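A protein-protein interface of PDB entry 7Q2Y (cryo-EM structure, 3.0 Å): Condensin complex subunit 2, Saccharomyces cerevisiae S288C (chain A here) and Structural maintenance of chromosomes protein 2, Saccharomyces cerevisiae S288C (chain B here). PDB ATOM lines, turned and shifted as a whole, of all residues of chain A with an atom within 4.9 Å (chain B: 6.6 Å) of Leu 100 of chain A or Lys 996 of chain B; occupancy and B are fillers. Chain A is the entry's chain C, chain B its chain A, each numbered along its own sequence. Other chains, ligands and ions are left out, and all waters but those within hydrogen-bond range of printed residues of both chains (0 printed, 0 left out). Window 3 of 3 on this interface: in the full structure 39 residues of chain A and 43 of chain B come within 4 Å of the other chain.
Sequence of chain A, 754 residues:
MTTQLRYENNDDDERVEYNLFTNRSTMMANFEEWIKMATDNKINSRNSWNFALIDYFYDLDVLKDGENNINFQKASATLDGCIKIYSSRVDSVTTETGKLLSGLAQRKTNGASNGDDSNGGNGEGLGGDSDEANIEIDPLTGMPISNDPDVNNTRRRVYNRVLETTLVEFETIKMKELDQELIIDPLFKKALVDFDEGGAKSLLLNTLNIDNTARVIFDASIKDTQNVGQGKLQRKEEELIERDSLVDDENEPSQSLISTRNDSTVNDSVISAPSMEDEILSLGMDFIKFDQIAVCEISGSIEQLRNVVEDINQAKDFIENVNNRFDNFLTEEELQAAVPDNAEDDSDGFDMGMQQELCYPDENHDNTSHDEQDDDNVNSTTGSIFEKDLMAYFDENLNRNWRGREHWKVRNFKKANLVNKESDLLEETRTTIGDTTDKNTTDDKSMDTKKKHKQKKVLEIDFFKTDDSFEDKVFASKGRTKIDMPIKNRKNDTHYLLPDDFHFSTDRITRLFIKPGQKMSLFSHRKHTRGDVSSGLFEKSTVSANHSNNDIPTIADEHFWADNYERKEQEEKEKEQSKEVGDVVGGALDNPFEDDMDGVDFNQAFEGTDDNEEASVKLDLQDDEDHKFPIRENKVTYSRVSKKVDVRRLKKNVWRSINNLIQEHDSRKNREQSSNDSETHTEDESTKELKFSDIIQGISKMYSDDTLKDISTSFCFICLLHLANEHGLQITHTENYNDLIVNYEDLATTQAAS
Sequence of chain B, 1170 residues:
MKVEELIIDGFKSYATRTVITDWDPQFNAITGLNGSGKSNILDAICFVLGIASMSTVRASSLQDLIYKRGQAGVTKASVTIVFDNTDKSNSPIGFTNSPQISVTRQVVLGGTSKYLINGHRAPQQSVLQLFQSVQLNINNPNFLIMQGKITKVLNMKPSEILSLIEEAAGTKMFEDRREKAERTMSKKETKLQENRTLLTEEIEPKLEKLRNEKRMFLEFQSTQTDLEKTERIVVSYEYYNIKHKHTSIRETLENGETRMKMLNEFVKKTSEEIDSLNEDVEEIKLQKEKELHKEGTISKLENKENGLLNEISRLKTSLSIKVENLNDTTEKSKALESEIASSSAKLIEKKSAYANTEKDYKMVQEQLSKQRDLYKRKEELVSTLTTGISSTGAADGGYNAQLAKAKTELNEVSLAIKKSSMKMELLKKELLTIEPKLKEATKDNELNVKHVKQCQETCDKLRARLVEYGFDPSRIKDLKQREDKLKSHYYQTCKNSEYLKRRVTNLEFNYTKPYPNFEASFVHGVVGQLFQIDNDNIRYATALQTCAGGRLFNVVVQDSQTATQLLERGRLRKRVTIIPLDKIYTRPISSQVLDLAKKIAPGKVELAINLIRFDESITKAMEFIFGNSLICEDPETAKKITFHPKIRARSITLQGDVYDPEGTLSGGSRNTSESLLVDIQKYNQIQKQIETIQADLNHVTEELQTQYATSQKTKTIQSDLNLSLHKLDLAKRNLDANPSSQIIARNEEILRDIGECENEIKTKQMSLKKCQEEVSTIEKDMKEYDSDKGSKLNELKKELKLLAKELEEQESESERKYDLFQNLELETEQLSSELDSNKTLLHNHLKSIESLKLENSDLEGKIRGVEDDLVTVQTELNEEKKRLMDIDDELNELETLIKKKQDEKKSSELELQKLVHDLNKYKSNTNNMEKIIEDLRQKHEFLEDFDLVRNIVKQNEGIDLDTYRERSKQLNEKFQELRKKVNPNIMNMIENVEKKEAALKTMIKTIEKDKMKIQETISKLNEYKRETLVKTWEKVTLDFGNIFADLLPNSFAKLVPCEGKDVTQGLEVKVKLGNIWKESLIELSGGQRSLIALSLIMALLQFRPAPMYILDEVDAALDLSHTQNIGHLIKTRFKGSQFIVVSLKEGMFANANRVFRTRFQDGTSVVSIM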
ATOM      1  N   GLU A  96      -7.009   2.857  -8.802  1.00  0.00           N
ATOM      2  CA  GLU A  96      -7.010   1.496  -8.271  1.00  0.00           C
ATOM      3  C   GLU A  96      -8.429   0.956  -8.135  1.00  0.00           C
ATOM      4  O   GLU A  96      -8.687  -0.216  -8.434  1.00  0.00           O
ATOM      5  CB  GLU A  96      -6.283   1.449  -6.929  1.00  0.00           C
ATOM      6  CG  GLU A  96      -4.780   1.655  -7.028  1.00  0.00           C
ATOM      7  CD  GLU A  96      -4.082   0.523  -7.758  1.00  0.00           C
ATOM      8  OE1 GLU A  96      -4.552  -0.630  -7.658  1.00  0.00           O
ATOM      9  OE2 GLU A  96      -3.065   0.787  -8.432  1.00  0.00           O
ATOM     10  N   THR A  97      -9.365   1.797  -7.686  1.00  0.00           N
ATOM     11  CA  THR A  97     -10.763   1.380  -7.625  1.00  0.00           C
ATOM     12  C   THR A  97     -11.307   1.086  -9.019  1.00  0.00           C
ATOM     13  O   THR A  97     -12.048   0.114  -9.217  1.00  0.00           O
ATOM     14  CB  THR A  97     -11.599   2.458  -6.933  1.00  0.00           C
ATOM     15  OG1 THR A  97     -11.109   2.661  -5.601  1.00  0.00           O
ATOM     16  CG2 THR A  97     -13.059   2.046  -6.866  1.00  0.00           C
ATOM     17  N   GLY A  98     -10.953   1.921  -9.997  1.00  0.00           N
ATOM     18  CA  GLY A  98     -11.344   1.643 -11.369  1.00  0.00           C
ATOM     19  C   GLY A  98     -10.799   0.318 -11.865  1.00  0.00           C
ATOM     20  O   GLY A  98     -11.496  -0.435 -12.546  1.00  0.00           O
ATOM     21  N   LYS A  99      -9.547   0.013 -11.517  1.00  0.00           N
ATOM     22  CA  LYS A  99      -8.972  -1.286 -11.853  1.00  0.00           C
ATOM     23  C   LYS A  99      -9.753  -2.419 -11.202  1.00  0.00           C
ATOM     24  O   LYS A  99      -9.993  -3.460 -11.826  1.00  0.00           O
ATOM     25  CB  LYS A  99      -7.507  -1.338 -11.419  1.00  0.00           C
ATOM     26  CG  LYS A  99      -6.515  -0.928 -12.489  1.00  0.00           C
ATOM     27  CD  LYS A  99      -5.093  -1.251 -12.059  1.00  0.00           C
ATOM     28  CE  LYS A  99      -4.156  -0.083 -12.316  1.00  0.00           C
ATOM     29  NZ  LYS A  99      -2.747  -0.413 -11.962  1.00  0.00           N
ATOM     30  N   LEU A 100     -10.146  -2.241  -9.937  1.00  0.00           N
ATOM     31  CA  LEU A 100     -10.905  -3.277  -9.241  1.00  0.00           C
ATOM     32  C   LEU A 100     -12.242  -3.545  -9.921  1.00  0.00           C
ATOM     33  O   LEU A 100     -12.617  -4.705 -10.123  1.00  0.00           O
ATOM     34  CB  LEU A 100     -11.123  -2.885  -7.781  1.00  0.00           C
ATOM     35  CG  LEU A 100      -9.865  -2.815  -6.922  1.00  0.00           C
ATOM     36  CD1 LEU A 100     -10.187  -2.284  -5.538  1.00  0.00           C
ATOM     37  CD2 LEU A 100      -9.248  -4.193  -6.839  1.00  0.00           C
ATOM     38  N   LEU A 101     -12.977  -2.489 -10.277  1.00  0.00           N
ATOM     39  CA  LEU A 101     -14.245  -2.697 -10.974  1.00  0.00           C
ATOM     40  C   LEU A 101     -14.033  -3.256 -12.377  1.00  0.00           C
ATOM     41  O   LEU A 101     -14.866  -4.020 -12.877  1.00  0.00           O
ATOM     42  CB  LEU A 101     -15.070  -1.408 -11.022  1.00  0.00           C
ATOM     43  CG  LEU A 101     -15.841  -0.985  -9.763  1.00  0.00           C
ATOM     44  CD1 LEU A 101     -14.960  -0.488  -8.635  1.00  0.00           C
ATOM     45  CD2 LEU A 101     -16.888   0.062 -10.121  1.00  0.00           C
ATOM     46  N   SER A 102     -12.929  -2.886 -13.031  1.00  0.00           N
ATOM     47  CA  SER A 102     -12.642  -3.440 -14.351  1.00  0.00           C
ATOM     48  C   SER A 102     -12.375  -4.937 -14.276  1.00  0.00           C
ATOM     49  O   SER A 102     -12.824  -5.701 -15.139  1.00  0.00           O
ATOM     50  CB  SER A 102     -11.454  -2.712 -14.979  1.00  0.00           C
ATOM     51  OG  SER A 102     -11.369  -2.978 -16.368  1.00  0.00           O
ATOM     52  N   GLY A 103     -11.641  -5.377 -13.251  1.00  0.00           N
ATOM     53  CA  GLY A 103     -11.332  -6.788 -13.109  1.00  0.00           C
ATOM     54  C   GLY A 103     -12.452  -7.628 -12.533  1.00  0.00           C
ATOM     55  O   GLY A 103     -12.394  -8.858 -12.619  1.00  0.00           O
ATOM     56  N   LEU A 104     -13.467  -6.994 -11.945  1.00  0.00           N
ATOM     57  CA  LEU A 104     -14.597  -7.707 -11.371  1.00  0.00           C
ATOM     58  C   LEU A 104     -15.865  -7.609 -12.207  1.00  0.00           C
ATOM     59  O   LEU A 104     -16.850  -8.282 -11.882  1.00  0.00           O
ATOM     60  CB  LEU A 104     -14.889  -7.191  -9.953  1.00  0.00           C
ATOM     61  CG  LEU A 104     -13.901  -7.603  -8.860  1.00  0.00           C
ATOM     62  CD1 LEU A 104     -14.138  -6.798  -7.592  1.00  0.00           C
ATOM     63  CD2 LEU A 104     -14.004  -9.094  -8.578  1.00  0.00           C
ATOM     64  N   LEU B 199     -16.922   1.136  -3.239  1.00  0.00           N
ATOM     65  CA  LEU B 199     -16.287   0.028  -2.531  1.00  0.00           C
ATOM     66  C   LEU B 199     -17.287  -0.715  -1.652  1.00  0.00           C
ATOM     67  O   LEU B 199     -17.292  -1.951  -1.611  1.00  0.00           O
ATOM     68  CB  LEU B 199     -15.119   0.546  -1.692  1.00  0.00           C
ATOM     69  CG  LEU B 199     -14.380  -0.467  -0.814  1.00  0.00           C
ATOM     70  CD1 LEU B 199     -13.802  -1.599  -1.654  1.00  0.00           C
ATOM     71  CD2 LEU B 199     -13.291   0.222  -0.007  1.00  0.00           C
ATOM     72  N   ILE B 203     -18.739  -3.730  -4.721  1.00  0.00           N
ATOM     73  CA  ILE B 203     -17.629  -4.673  -4.613  1.00  0.00           C
ATOM     74  C   ILE B 203     -17.923  -5.739  -3.561  1.00  0.00           C
ATOM     75  O   ILE B 203     -17.614  -6.921  -3.751  1.00  0.00           O
ATOM     76  CB  ILE B 203     -16.319  -3.921  -4.318  1.00  0.00           C
ATOM     77  CG1 ILE B 203     -15.968  -2.995  -5.484  1.00  0.00           C
ATOM     78  CG2 ILE B 203     -15.189  -4.894  -4.071  1.00  0.00           C
ATOM     79  CD1 ILE B 203     -14.836  -2.038  -5.189  1.00  0.00           C
ATOM     80  N   GLU B 991      -7.780 -14.384  -4.648  1.00  0.00           N
ATOM     81  CA  GLU B 991      -6.619 -13.962  -3.870  1.00  0.00           C
ATOM     82  C   GLU B 991      -6.120 -12.595  -4.323  1.00  0.00           C
ATOM     83  O   GLU B 991      -5.823 -11.725  -3.493  1.00  0.00           O
ATOM     84  CB  GLU B 991      -5.510 -15.007  -3.980  1.00  0.00           C
ATOM     85  CG  GLU B 991      -5.593 -16.107  -2.935  1.00  0.00           C
ATOM     86  CD  GLU B 991      -5.211 -17.466  -3.488  1.00  0.00           C
ATOM     87  OE1 GLU B 991      -4.692 -17.523  -4.623  1.00  0.00           O
ATOM     88  OE2 GLU B 991      -5.431 -18.477  -2.788  1.00  0.00           O
ATOM     89  N   ASN B 992      -6.031 -12.386  -5.640  1.00  0.00           N
ATOM     90  CA  ASN B 992      -5.606 -11.088  -6.152  1.00  0.00           C
ATOM     91  C   ASN B 992      -6.589  -9.993  -5.759  1.00  0.00           C
ATOM     92  O   ASN B 992      -6.180  -8.890  -5.373  1.00  0.00           O
ATOM     93  CB  ASN B 992      -5.448 -11.147  -7.672  1.00  0.00           C
ATOM     94  CG  ASN B 992      -4.365 -12.114  -8.107  1.00  0.00           C
ATOM     95  OD1 ASN B 992      -3.783 -12.824  -7.286  1.00  0.00           O
ATOM     96  ND2 ASN B 992      -4.087 -12.146  -9.405  1.00  0.00           N
ATOM     97  N   VAL B 993      -7.890 -10.281  -5.845  1.00  0.00           N
ATOM     98  CA  VAL B 993      -8.898  -9.293  -5.476  1.00  0.00           C
ATOM     99  C   VAL B 993      -8.776  -8.931  -4.001  1.00  0.00           C
ATOM    100  O   VAL B 993      -8.837  -7.753  -3.632  1.00  0.00           O
ATOM    101  CB  VAL B 993     -10.306  -9.813  -5.823  1.00  0.00           C
ATOM    102  CG1 VAL B 993     -11.369  -8.982  -5.127  1.00  0.00           C
ATOM    103  CG2 VAL B 993     -10.519  -9.791  -7.327  1.00  0.00           C
ATOM    104  N   GLU B 994      -8.594  -9.933  -3.136  1.00  0.00           N
ATOM    105  CA  GLU B 994      -8.454  -9.662  -1.709  1.00  0.00           C
ATOM    106  C   GLU B 994      -7.210  -8.829  -1.420  1.00  0.00           C
ATOM    107  O   GLU B 994      -7.257  -7.889  -0.617  1.00  0.00           O
ATOM    108  CB  GLU B 994      -8.415 -10.975  -0.928  1.00  0.00           C
ATOM    109  CG  GLU B 994      -9.762 -11.674  -0.826  1.00  0.00           C
ATOM    110  CD  GLU B 994      -9.674 -13.005  -0.107  1.00  0.00           C
ATOM    111  OE1 GLU B 994      -8.546 -13.446   0.198  1.00  0.00           O
ATOM    112  OE2 GLU B 994     -10.735 -13.612   0.156  1.00  0.00           O
ATOM    113  N   LYS B 995      -6.088  -9.157  -2.067  1.00  0.00           N
ATOM    114  CA  LYS B 995      -4.863  -8.390  -1.850  1.00  0.00           C
ATOM    115  C   LYS B 995      -5.034  -6.941  -2.291  1.00  0.00           C
ATOM    116  O   LYS B 995      -4.637  -6.007  -1.580  1.00  0.00           O
ATOM    117  CB  LYS B 995      -3.697  -9.047  -2.590  1.00  0.00           C
ATOM    118  CG  LYS B 995      -3.249 -10.371  -1.995  1.00  0.00           C
ATOM    119  CD  LYS B 995      -2.200 -11.040  -2.867  1.00  0.00           C
ATOM    120  CE  LYS B 995      -0.881 -10.287  -2.820  1.00  0.00           C
ATOM    121  NZ  LYS B 995       0.187 -10.994  -3.580  1.00  0.00           N
ATOM    122  N   LYS B 996      -5.639  -6.732  -3.463  1.00  0.00           N
ATOM    123  CA  LYS B 996      -5.828  -5.372  -3.957  1.00  0.00           C
ATOM    124  C   LYS B 996      -6.798  -4.591  -3.078  1.00  0.00           C
ATOM    125  O   LYS B 996      -6.612  -3.389  -2.853  1.00  0.00           O
ATOM    126  CB  LYS B 996      -6.310  -5.401  -5.406  1.00  0.00           C
ATOM    127  CG  LYS B 996      -5.335  -6.048  -6.377  1.00  0.00           C
ATOM    128  CD  LYS B 996      -4.315  -5.048  -6.891  1.00  0.00           C
ATOM    129  CE  LYS B 996      -3.215  -5.741  -7.678  1.00  0.00           C
ATOM    130  NZ  LYS B 996      -2.440  -6.688  -6.831  1.00  0.00           N
ATOM    131  N   GLU B 997      -7.842  -5.253  -2.570  1.00  0.00           N
ATOM    132  CA  GLU B 997      -8.773  -4.581  -1.669  1.00  0.00           C
ATOM    133  C   GLU B 997      -8.098  -4.195  -0.360  1.00  0.00           C
ATOM    134  O   GLU B 997      -8.355  -3.111   0.181  1.00  0.00           O
ATOM    135  CB  GLU B 997      -9.984  -5.472  -1.409  1.00  0.00           C
ATOM    136  CG  GLU B 997     -10.899  -5.616  -2.607  1.00  0.00           C
ATOM    137  CD  GLU B 997     -11.951  -6.682  -2.406  1.00  0.00           C
ATOM    138  OE1 GLU B 997     -11.876  -7.412  -1.396  1.00  0.00           O
ATOM    139  OE2 GLU B 997     -12.848  -6.794  -3.264  1.00  0.00           O
ATOM    140  N   ALA B 998      -7.241  -5.070   0.172  1.00  0.00           N
ATOM    141  CA  ALA B 998      -6.487  -4.719   1.371  1.00  0.00           C
ATOM    142  C   ALA B 998      -5.587  -3.518   1.117  1.00  0.00           C
ATOM    143  O   ALA B 998      -5.495  -2.609   1.954  1.00  0.00           O
ATOM    144  CB  ALA B 998      -5.668  -5.919   1.848  1.00  0.00           C
ATOM    145  N   ALA B 999      -4.919  -3.494  -0.040  1.00  0.00           N
ATOM    146  CA  ALA B 999      -4.085  -2.346  -0.386  1.00  0.00           C
ATOM    147  C   ALA B 999      -4.913  -1.069  -0.482  1.00  0.00           C
ATOM    148  O   ALA B 999      -4.490  -0.006  -0.007  1.00  0.00           O
ATOM    149  CB  ALA B 999      -3.348  -2.610  -1.699  1.00  0.00           C
ATOM    150  N   LEU B1000      -6.097  -1.155  -1.093  1.00  0.00           N
ATOM    151  CA  LEU B1000      -6.962   0.014  -1.215  1.00  0.00           C
ATOM    152  C   LEU B1000      -7.405   0.522   0.152  1.00  0.00           C
ATOM    153  O   LEU B1000      -7.419   1.735   0.397  1.00  0.00           O
ATOM    154  CB  LEU B1000      -8.176  -0.319  -2.081  1.00  0.00           C
ATOM    155  CG  LEU B1000      -9.128   0.843  -2.373  1.00  0.00           C
ATOM    156  CD1 LEU B1000      -8.443   1.885  -3.242  1.00  0.00           C
ATOM    157  CD2 LEU B1000     -10.409   0.349  -3.024  1.00  0.00           C
ATOM    158  N   LYS B1001      -7.775  -0.392   1.052  1.00  0.00           N
ATOM    159  CA  LYS B1001      -8.180   0.017   2.394  1.00  0.00           C
ATOM    160  C   LYS B1001      -7.029   0.678   3.141  1.00  0.00           C
ATOM    161  O   LYS B1001      -7.226   1.688   3.834  1.00  0.00           O
ATOM    162  CB  LYS B1001      -8.708  -1.187   3.174  1.00  0.00           C
ATOM    163  CG  LYS B1001      -9.996  -1.770   2.615  1.00  0.00           C
ATOM    164  CD  LYS B1001     -10.474  -2.950   3.442  1.00  0.00           C
ATOM    165  CE  LYS B1001     -11.808  -3.473   2.935  1.00  0.00           C
ATOM    166  NZ  LYS B1001     -11.690  -4.075   1.579  1.00  0.00           N
ATOM    167  N   MET B1003      -4.503   2.309   1.790  1.00  0.00           N
ATOM    168  CA  MET B1003      -4.299   3.632   1.205  1.00  0.00           C
ATOM    169  C   MET B1003      -5.357   4.619   1.682  1.00  0.00           C
ATOM    170  O   MET B1003      -5.046   5.779   1.970  1.00  0.00           O
ATOM    171  CB  MET B1003      -4.280   3.553  -0.322  1.00  0.00           C
ATOM    172  CG  MET B1003      -3.093   2.791  -0.891  1.00  0.00           C
ATOM    173  SD  MET B1003      -3.051   2.770  -2.696  1.00  0.00           S
ATOM    174  CE  MET B1003      -4.358   1.611  -3.072  1.00  0.00           C
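Of chain A, only Leu 100 comes within 4 Å of Lys 996 of chain B. Printed residues of chain B within 4 Å of Glu 96 of chain A: Met 1003. Printed residues of chain A within 4 Å of Met 1003 of chain B: Glu 96. Of the printed residues of chain A, Val 993 of chain B touches Leu 104. Printed residues of chain B within 4 Å of Leu 104 of chain A: Val 993 (3.8 Å). Asn 992 of chain B touches none of the printed residues of chain A. Ala 998 of chain B touches none of the printed residues of chain A. The nearest residue of chain B that does not touch Leu 100 of chain A is Glu 997 of chain B (4.5 Å). The nearest printed residue of chain B that does not touch Glu 96 of chain A is Leu 1000 of chain B (4.3 Å).
Among the printed residues, merely in contact across the chains: Glu 96 of chain A with Met 1003 of chain B (3.98 Å), Thr 97 of chain A with Leu 1000 of chain B (3.5 Å), Leu 100 of chain A with Lys 996 of chain B (3.5 Å), Leu 100 of chain A with Leu 1000 of chain B (3.6 Å), Leu 101 of chain A with Ile 203 of chain B (3.8 Å) and Leu 104 of chain A with Val 993 of chain B (3.8 Å).
Of the 14 printed residues of chain B, 5 touch a printed residue of chain A. Hydrophobic or aromatic side chains of chain B within 4 Å of the printed part of chain A: Ile 203, Val 993, Leu 1000 and Met 1003. Along chain B the printed residues that touch a printed residue of chain A span positions 203 to 1003. Among the printed residues, 6 pairs touch across the chains.
The side-chain amino group (NZ) of Lys 99 of chain A is in salt-bridge range of the side-chain carboxylate (OE2) of Glu 96 of chain A, 3.7 Å away.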
